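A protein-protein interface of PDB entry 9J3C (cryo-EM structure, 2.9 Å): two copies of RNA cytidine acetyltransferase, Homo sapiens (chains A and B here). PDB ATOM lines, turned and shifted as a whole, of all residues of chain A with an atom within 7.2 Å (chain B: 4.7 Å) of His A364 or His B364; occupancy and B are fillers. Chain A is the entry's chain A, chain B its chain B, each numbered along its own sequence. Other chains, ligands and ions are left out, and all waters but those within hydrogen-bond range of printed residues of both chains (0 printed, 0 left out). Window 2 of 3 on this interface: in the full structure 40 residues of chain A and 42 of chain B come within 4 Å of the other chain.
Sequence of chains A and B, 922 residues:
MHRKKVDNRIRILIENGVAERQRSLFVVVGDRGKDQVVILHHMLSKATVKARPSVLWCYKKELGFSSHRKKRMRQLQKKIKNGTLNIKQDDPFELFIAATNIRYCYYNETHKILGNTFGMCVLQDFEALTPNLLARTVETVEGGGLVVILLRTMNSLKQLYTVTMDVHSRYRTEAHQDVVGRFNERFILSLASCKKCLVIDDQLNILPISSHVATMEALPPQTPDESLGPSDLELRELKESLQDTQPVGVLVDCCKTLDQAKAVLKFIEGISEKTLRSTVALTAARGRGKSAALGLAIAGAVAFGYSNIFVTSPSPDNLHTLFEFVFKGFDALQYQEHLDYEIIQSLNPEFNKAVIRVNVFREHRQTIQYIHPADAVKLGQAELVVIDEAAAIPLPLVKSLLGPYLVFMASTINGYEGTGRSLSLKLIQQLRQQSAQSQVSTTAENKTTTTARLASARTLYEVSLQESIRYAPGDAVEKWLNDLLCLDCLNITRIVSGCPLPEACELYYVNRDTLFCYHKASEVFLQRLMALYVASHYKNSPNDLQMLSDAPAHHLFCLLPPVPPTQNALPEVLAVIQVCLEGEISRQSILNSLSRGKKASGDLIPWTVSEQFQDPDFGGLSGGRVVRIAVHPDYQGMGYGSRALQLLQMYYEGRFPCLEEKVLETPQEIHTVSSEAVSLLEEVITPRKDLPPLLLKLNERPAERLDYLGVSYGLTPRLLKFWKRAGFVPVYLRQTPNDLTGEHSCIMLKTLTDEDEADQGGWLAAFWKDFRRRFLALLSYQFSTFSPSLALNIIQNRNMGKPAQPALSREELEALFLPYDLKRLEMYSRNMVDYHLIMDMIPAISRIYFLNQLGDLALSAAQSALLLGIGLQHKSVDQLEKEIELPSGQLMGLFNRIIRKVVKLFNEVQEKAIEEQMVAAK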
ATOM      1  N   LYS A 274      -1.519 -13.383  -6.828  1.00  0.00           N
ATOM      2  CA  LYS A 274      -0.974 -13.796  -8.121  1.00  0.00           C
ATOM      3  C   LYS A 274      -2.033 -13.669  -9.221  1.00  0.00           C
ATOM      4  O   LYS A 274      -2.460 -14.642  -9.842  1.00  0.00           O
ATOM      5  CB  LYS A 274      -0.431 -15.216  -8.032  1.00  0.00           C
ATOM      6  CG  LYS A 274       0.854 -15.335  -7.225  1.00  0.00           C
ATOM      7  CD  LYS A 274       2.067 -14.924  -8.045  1.00  0.00           C
ATOM      8  CE  LYS A 274       2.138 -15.685  -9.358  1.00  0.00           C
ATOM      9  NZ  LYS A 274       3.061 -15.032 -10.327  1.00  0.00           N
ATOM     10  N   VAL A 302      10.493  -9.157  -6.988  1.00  0.00           N
ATOM     11  CA  VAL A 302      11.585 -10.097  -7.225  1.00  0.00           C
ATOM     12  C   VAL A 302      11.598 -11.178  -6.151  1.00  0.00           C
ATOM     13  O   VAL A 302      11.739 -12.370  -6.450  1.00  0.00           O
ATOM     14  CB  VAL A 302      12.928  -9.346  -7.295  1.00  0.00           C
ATOM     15  CG1 VAL A 302      14.085 -10.272  -6.945  1.00  0.00           C
ATOM     16  CG2 VAL A 302      13.125  -8.737  -8.674  1.00  0.00           C
ATOM     17  N   PHE A 304       9.093 -12.167  -4.548  1.00  0.00           N
ATOM     18  CA  PHE A 304       7.833 -12.895  -4.616  1.00  0.00           C
ATOM     19  C   PHE A 304       7.796 -13.917  -5.746  1.00  0.00           C
ATOM     20  O   PHE A 304       6.763 -14.566  -5.940  1.00  0.00           O
ATOM     21  CB  PHE A 304       6.665 -11.916  -4.769  1.00  0.00           C
ATOM     22  CG  PHE A 304       5.858 -11.734  -3.515  1.00  0.00           C
ATOM     23  CD1 PHE A 304       4.905 -12.669  -3.148  1.00  0.00           C
ATOM     24  CD2 PHE A 304       6.055 -10.629  -2.703  1.00  0.00           C
ATOM     25  CE1 PHE A 304       4.162 -12.505  -1.994  1.00  0.00           C
ATOM     26  CE2 PHE A 304       5.315 -10.460  -1.549  1.00  0.00           C
ATOM     27  CZ  PHE A 304       4.367 -11.399  -1.194  1.00  0.00           C
ATOM     28  N   GLY A 305       8.887 -14.074  -6.493  1.00  0.00           N
ATOM     29  CA  GLY A 305       8.960 -15.050  -7.558  1.00  0.00           C
ATOM     30  C   GLY A 305       8.698 -14.520  -8.950  1.00  0.00           C
ATOM     31  O   GLY A 305       8.683 -15.314  -9.900  1.00  0.00           O
ATOM     32  N   TYR A 306       8.488 -13.216  -9.107  1.00  0.00           N
ATOM     33  CA  TYR A 306       8.267 -12.650 -10.429  1.00  0.00           C
ATOM     34  C   TYR A 306       9.535 -12.749 -11.268  1.00  0.00           C
ATOM     35  O   TYR A 306      10.638 -12.457 -10.797  1.00  0.00           O
ATOM     36  CB  TYR A 306       7.820 -11.192 -10.319  1.00  0.00           C
ATOM     37  CG  TYR A 306       6.334 -11.023 -10.091  1.00  0.00           C
ATOM     38  CD1 TYR A 306       5.748 -11.404  -8.892  1.00  0.00           C
ATOM     39  CD2 TYR A 306       5.519 -10.485 -11.078  1.00  0.00           C
ATOM     40  CE1 TYR A 306       4.390 -11.252  -8.680  1.00  0.00           C
ATOM     41  CE2 TYR A 306       4.161 -10.329 -10.876  1.00  0.00           C
ATOM     42  CZ  TYR A 306       3.602 -10.713  -9.675  1.00  0.00           C
ATOM     43  OH  TYR A 306       2.250 -10.560  -9.469  1.00  0.00           O
ATOM     44  N   SER A 307       9.373 -13.166 -12.524  1.00  0.00           N
ATOM     45  CA  SER A 307      10.498 -13.370 -13.426  1.00  0.00           C
ATOM     46  C   SER A 307      10.637 -12.297 -14.493  1.00  0.00           C
ATOM     47  O   SER A 307      11.759 -12.010 -14.915  1.00  0.00           O
ATOM     48  CB  SER A 307      10.385 -14.736 -14.116  1.00  0.00           C
ATOM     49  OG  SER A 307      10.001 -15.742 -13.195  1.00  0.00           O
ATOM     50  N   VAL A 360      18.812 -11.690 -11.395  1.00  0.00           N
ATOM     51  CA  VAL A 360      18.776 -12.289 -10.066  1.00  0.00           C
ATOM     52  C   VAL A 360      18.608 -13.793 -10.226  1.00  0.00           C
ATOM     53  O   VAL A 360      17.690 -14.250 -10.916  1.00  0.00           O
ATOM     54  CB  VAL A 360      17.641 -11.701  -9.207  1.00  0.00           C
ATOM     55  CG1 VAL A 360      17.687 -12.279  -7.801  1.00  0.00           C
ATOM     56  CG2 VAL A 360      17.732 -10.184  -9.170  1.00  0.00           C
ATOM     57  N   PHE A 361      19.495 -14.558  -9.589  1.00  0.00           N
ATOM     58  CA  PHE A 361      19.480 -16.021  -9.657  1.00  0.00           C
ATOM     59  C   PHE A 361      19.575 -16.575  -8.237  1.00  0.00           C
ATOM     60  O   PHE A 361      20.668 -16.861  -7.742  1.00  0.00           O
ATOM     61  CB  PHE A 361      20.612 -16.542 -10.544  1.00  0.00           C
ATOM     62  CG  PHE A 361      21.802 -15.625 -10.617  1.00  0.00           C
ATOM     63  CD1 PHE A 361      21.903 -14.675 -11.621  1.00  0.00           C
ATOM     64  CD2 PHE A 361      22.823 -15.717  -9.685  1.00  0.00           C
ATOM     65  CE1 PHE A 361      22.996 -13.832 -11.691  1.00  0.00           C
ATOM     66  CE2 PHE A 361      23.918 -14.876  -9.749  1.00  0.00           C
ATOM     67  CZ  PHE A 361      24.005 -13.933 -10.754  1.00  0.00           C
ATOM     68  N   ARG A 362      18.423 -16.726  -7.583  1.00  0.00           N
ATOM     69  CA  ARG A 362      18.346 -17.346  -6.266  1.00  0.00           C
ATOM     70  C   ARG A 362      17.748 -18.745  -6.339  1.00  0.00           C
ATOM     71  O   ARG A 362      18.367 -19.712  -5.886  1.00  0.00           O
ATOM     72  CB  ARG A 362      17.529 -16.461  -5.314  1.00  0.00           C
ATOM     73  CG  ARG A 362      18.234 -15.178  -4.906  1.00  0.00           C
ATOM     74  CD  ARG A 362      18.460 -15.129  -3.404  1.00  0.00           C
ATOM     75  NE  ARG A 362      17.312 -15.631  -2.661  1.00  0.00           N
ATOM     76  CZ  ARG A 362      17.367 -16.103  -1.424  1.00  0.00           C
ATOM     77  NH1 ARG A 362      18.508 -16.152  -0.754  1.00  0.00           N
ATOM     78  NH2 ARG A 362      16.252 -16.535  -0.843  1.00  0.00           N
ATOM     79  N   GLU A 363      16.549 -18.876  -6.903  1.00  0.00           N
ATOM     80  CA  GLU A 363      15.938 -20.170  -7.178  1.00  0.00           C
ATOM     81  C   GLU A 363      15.744 -20.398  -8.668  1.00  0.00           C
ATOM     82  O   GLU A 363      16.155 -21.440  -9.192  1.00  0.00           O
ATOM     83  CB  GLU A 363      14.591 -20.288  -6.445  1.00  0.00           C
ATOM     84  N   HIS A 364      15.130 -19.448  -9.362  1.00  0.00           N
ATOM     85  CA  HIS A 364      15.031 -19.440 -10.814  1.00  0.00           C
ATOM     86  C   HIS A 364      15.725 -18.183 -11.338  1.00  0.00           C
ATOM     87  O   HIS A 364      16.354 -17.436 -10.584  1.00  0.00           O
ATOM     88  CB  HIS A 364      13.568 -19.519 -11.260  1.00  0.00           C
ATOM     89  CG  HIS A 364      12.641 -18.667 -10.448  1.00  0.00           C
ATOM     90  ND1 HIS A 364      12.166 -19.050  -9.212  1.00  0.00           N
ATOM     91  CD2 HIS A 364      12.096 -17.453 -10.701  1.00  0.00           C
ATOM     92  CE1 HIS A 364      11.372 -18.108  -8.737  1.00  0.00           C
ATOM     93  NE2 HIS A 364      11.312 -17.128  -9.620  1.00  0.00           N
ATOM     94  N   ARG A 365      15.611 -17.950 -12.641  1.00  0.00           N
ATOM     95  CA  ARG A 365      16.234 -16.799 -13.282  1.00  0.00           C
ATOM     96  C   ARG A 365      15.189 -15.711 -13.493  1.00  0.00           C
ATOM     97  O   ARG A 365      14.204 -15.919 -14.211  1.00  0.00           O
ATOM     98  CB  ARG A 365      16.880 -17.195 -14.610  1.00  0.00           C
ATOM     99  CG  ARG A 365      18.292 -16.656 -14.787  1.00  0.00           C
ATOM    100  CD  ARG A 365      19.003 -17.321 -15.953  1.00  0.00           C
ATOM    101  NE  ARG A 365      20.028 -18.256 -15.503  1.00  0.00           N
ATOM    102  CZ  ARG A 365      21.321 -17.971 -15.427  1.00  0.00           C
ATOM    103  NH1 ARG A 365      21.787 -16.780 -15.765  1.00  0.00           N
ATOM    104  NH2 ARG A 365      22.168 -18.904 -15.001  1.00  0.00           N
ATOM    105  N   GLN A 366      15.408 -14.557 -12.868  1.00  0.00           N
ATOM    106  CA  GLN A 366      14.544 -13.397 -13.010  1.00  0.00           C
ATOM    107  C   GLN A 366      15.375 -12.203 -13.458  1.00  0.00           C
ATOM    108  O   GLN A 366      16.541 -12.062 -13.078  1.00  0.00           O
ATOM    109  CB  GLN A 366      13.824 -13.064 -11.696  1.00  0.00           C
ATOM    110  CG  GLN A 366      13.529 -14.271 -10.821  1.00  0.00           C
ATOM    111  CD  GLN A 366      13.327 -13.898  -9.365  1.00  0.00           C
ATOM    112  OE1 GLN A 366      14.156 -14.213  -8.511  1.00  0.00           O
ATOM    113  NE2 GLN A 366      12.219 -13.224  -9.075  1.00  0.00           N
ATOM    114  N   GLU A 383       5.329  -9.875 -16.808  1.00  0.00           N
ATOM    115  CA  GLU A 383       4.505 -10.102 -15.628  1.00  0.00           C
ATOM    116  C   GLU A 383       4.227  -8.824 -14.851  1.00  0.00           C
ATOM    117  O   GLU A 383       3.090  -8.597 -14.427  1.00  0.00           O
ATOM    118  CB  GLU A 383       5.172 -11.124 -14.703  1.00  0.00           C
ATOM    119  CG  GLU A 383       4.925 -12.571 -15.094  1.00  0.00           C
ATOM    120  CD  GLU A 383       5.639 -13.549 -14.180  1.00  0.00           C
ATOM    121  OE1 GLU A 383       6.830 -13.832 -14.425  1.00  0.00           O
ATOM    122  OE2 GLU A 383       5.007 -14.032 -13.218  1.00  0.00           O
ATOM    123  N   GLY B 305      12.523 -25.533 -13.789  1.00  0.00           N
ATOM    124  CA  GLY B 305      12.441 -24.148 -13.378  1.00  0.00           C
ATOM    125  C   GLY B 305      12.608 -23.127 -14.481  1.00  0.00           C
ATOM    126  O   GLY B 305      12.585 -21.924 -14.191  1.00  0.00           O
ATOM    127  N   SER B 307      11.710 -20.553 -17.245  1.00  0.00           N
ATOM    128  CA  SER B 307      10.545 -19.695 -17.410  1.00  0.00           C
ATOM    129  C   SER B 307      10.345 -19.193 -18.831  1.00  0.00           C
ATOM    130  O   SER B 307       9.202 -18.978 -19.238  1.00  0.00           O
ATOM    131  CB  SER B 307      10.637 -18.486 -16.470  1.00  0.00           C
ATOM    132  OG  SER B 307      11.134 -18.865 -15.198  1.00  0.00           O
ATOM    133  N   VAL B 360       2.290 -22.453 -17.659  1.00  0.00           N
ATOM    134  CA  VAL B 360       2.443 -23.386 -16.549  1.00  0.00           C
ATOM    135  C   VAL B 360       2.616 -22.581 -15.271  1.00  0.00           C
ATOM    136  O   VAL B 360       3.465 -21.684 -15.206  1.00  0.00           O
ATOM    137  CB  VAL B 360       3.636 -24.336 -16.761  1.00  0.00           C
ATOM    138  CG1 VAL B 360       3.673 -25.394 -15.668  1.00  0.00           C
ATOM    139  CG2 VAL B 360       3.564 -24.984 -18.135  1.00  0.00           C
ATOM    140  N   PHE B 361       1.812 -22.899 -14.256  1.00  0.00           N
ATOM    141  CA  PHE B 361       1.852 -22.218 -12.960  1.00  0.00           C
ATOM    142  C   PHE B 361       1.818 -23.273 -11.858  1.00  0.00           C
ATOM    143  O   PHE B 361       0.745 -23.663 -11.388  1.00  0.00           O
ATOM    144  CB  PHE B 361       0.703 -21.216 -12.828  1.00  0.00           C
ATOM    145  CG  PHE B 361      -0.514 -21.568 -13.640  1.00  0.00           C
ATOM    146  CD1 PHE B 361      -0.666 -21.083 -14.929  1.00  0.00           C
ATOM    147  CD2 PHE B 361      -1.506 -22.379 -13.115  1.00  0.00           C
ATOM    148  CE1 PHE B 361      -1.782 -21.402 -15.680  1.00  0.00           C
ATOM    149  CE2 PHE B 361      -2.625 -22.700 -13.861  1.00  0.00           C
ATOM    150  CZ  PHE B 361      -2.762 -22.211 -15.144  1.00  0.00           C
ATOM    151  N   ARG B 362       2.999 -23.731 -11.446  1.00  0.00           N
ATOM    152  CA  ARG B 362       3.140 -24.673 -10.342  1.00  0.00           C
ATOM    153  C   ARG B 362       3.843 -24.035  -9.151  1.00  0.00           C
ATOM    154  O   ARG B 362       3.314 -24.044  -8.036  1.00  0.00           O
ATOM    155  CB  ARG B 362       3.898 -25.923 -10.810  1.00  0.00           C
ATOM    156  CG  ARG B 362       2.998 -27.047 -11.301  1.00  0.00           C
ATOM    157  CD  ARG B 362       2.904 -28.168 -10.280  1.00  0.00           C
ATOM    158  NE  ARG B 362       4.209 -28.750  -9.986  1.00  0.00           N
ATOM    159  CZ  ARG B 362       4.414 -29.732  -9.120  1.00  0.00           C
ATOM    160  NH1 ARG B 362       3.416 -30.272  -8.439  1.00  0.00           N
ATOM    161  NH2 ARG B 362       5.650 -30.185  -8.932  1.00  0.00           N
ATOM    162  N   GLU B 363       5.034 -23.478  -9.362  1.00  0.00           N
ATOM    163  CA  GLU B 363       5.743 -22.699  -8.356  1.00  0.00           C
ATOM    164  C   GLU B 363       5.893 -21.243  -8.764  1.00  0.00           C
ATOM    165  O   GLU B 363       5.555 -20.341  -7.991  1.00  0.00           O
ATOM    166  CB  GLU B 363       7.125 -23.313  -8.086  1.00  0.00           C
ATOM    167  N   HIS B 364       6.393 -20.994  -9.969  1.00  0.00           N
ATOM    168  CA  HIS B 364       6.432 -19.671 -10.574  1.00  0.00           C
ATOM    169  C   HIS B 364       5.660 -19.720 -11.893  1.00  0.00           C
ATOM    170  O   HIS B 364       5.034 -20.728 -12.233  1.00  0.00           O
ATOM    171  CB  HIS B 364       7.877 -19.202 -10.768  1.00  0.00           C
ATOM    172  CG  HIS B 364       8.819 -20.294 -11.172  1.00  0.00           C
ATOM    173  ND1 HIS B 364       9.356 -21.186 -10.270  1.00  0.00           N
ATOM    174  CD2 HIS B 364       9.322 -20.634 -12.383  1.00  0.00           C
ATOM    175  CE1 HIS B 364      10.149 -22.030 -10.907  1.00  0.00           C
ATOM    176  NE2 HIS B 364      10.145 -21.717 -12.189  1.00  0.00           N
ATOM    177  N   ARG B 365       5.707 -18.622 -12.640  1.00  0.00           N
ATOM    178  CA  ARG B 365       5.009 -18.520 -13.916  1.00  0.00           C
ATOM    179  C   ARG B 365       5.995 -18.769 -15.051  1.00  0.00           C
ATOM    180  O   ARG B 365       6.961 -18.017 -15.217  1.00  0.00           O
ATOM    181  CB  ARG B 365       4.343 -17.153 -14.067  1.00  0.00           C
ATOM    182  CG  ARG B 365       3.349 -17.077 -15.216  1.00  0.00           C
ATOM    183  CD  ARG B 365       2.010 -17.684 -14.829  1.00  0.00           C
ATOM    184  NE  ARG B 365       1.351 -16.934 -13.765  1.00  0.00           N
ATOM    185  CZ  ARG B 365       0.087 -16.536 -13.801  1.00  0.00           C
ATOM    186  NH1 ARG B 365      -0.691 -16.801 -14.838  1.00  0.00           N
ATOM    187  NH2 ARG B 365      -0.409 -15.859 -12.770  1.00  0.00           N
ATOM    188  N   GLN B 366       5.747 -19.823 -15.823  1.00  0.00           N
ATOM    189  CA  GLN B 366       6.557 -20.172 -16.980  1.00  0.00           C
ATOM    190  C   GLN B 366       5.663 -20.302 -18.204  1.00  0.00           C
ATOM    191  O   GLN B 366       4.494 -20.687 -18.099  1.00  0.00           O
ATOM    192  CB  GLN B 366       7.323 -21.483 -16.755  1.00  0.00           C
ATOM    193  CG  GLN B 366       7.737 -21.729 -15.314  1.00  0.00           C
ATOM    194  CD  GLN B 366       7.934 -23.200 -15.007  1.00  0.00           C
ATOM    195  OE1 GLN B 366       7.111 -23.822 -14.338  1.00  0.00           O
ATOM    196  NE2 GLN B 366       9.031 -23.765 -15.498  1.00  0.00           N
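Among the printed residues, merely in contact across the chains: Glu A383 with Arg B365, His A364 with His B364, Lys A274 with Arg B365, Ser A307 with Ser B307 and His A364 with Gly B305.
Ser A307 touches its own counterpart, Ser B307. His A364 touches Gly B305, but with the chains exchanged Gly A305 does not touch His B364 (4.1 Å). His B364 touches its own counterpart, His A364. Of the 5 pairs that touch across the chains among the printed residues, 2 have their exchanged pair printed and touching as well.
N of Ser A307 sits at hydrogen-bond distance from OE1 of Glu A383, 3.2 Å away. The side-chain amino group (NZ) of Lys A274 is in salt-bridge range of the side-chain carboxylate (OE2) of Glu A383 (3.6 Å). The backbone carbonyl oxygen (O) of Gly A305 sits at hydrogen-bond distance from a ring nitrogen (NE2) of His A364 (3.2 Å). NE2 of His B364 lies within hydrogen-bond range of O of Gly B305, at 3.2 Å.
Of the printed residues of chain B, Lys A274 touches Arg B365. Gly A305 touches none of the printed residues of chain B. Of chain B, only Gly B305 (3.9 Å) and His B364 (3.7 Å) come within 4 Å of His A364. Of the printed residues of chain A, Ser B307 touches Ser A307. No residue of chain A comes within 4 Å of Glu B363. His B364 touches one residue of chain A. The nearest residue of chain A that does not touch His B364 is Gly A305 (4.1 Å). The nearest printed residue of chain A that does not touch Arg B365 is Ser A307 (4.3 Å).
Printed residues of chain B that touch a printed residue of chain A: Gly B305, Ser B307, His B364 and Arg B365. Among the printed residues, 5 pairs touch across the chains. Among the printed residues, no Asp or Glu carboxylate lies within 4 Å of a Lys or Arg side-chain nitrogen of the other chain.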
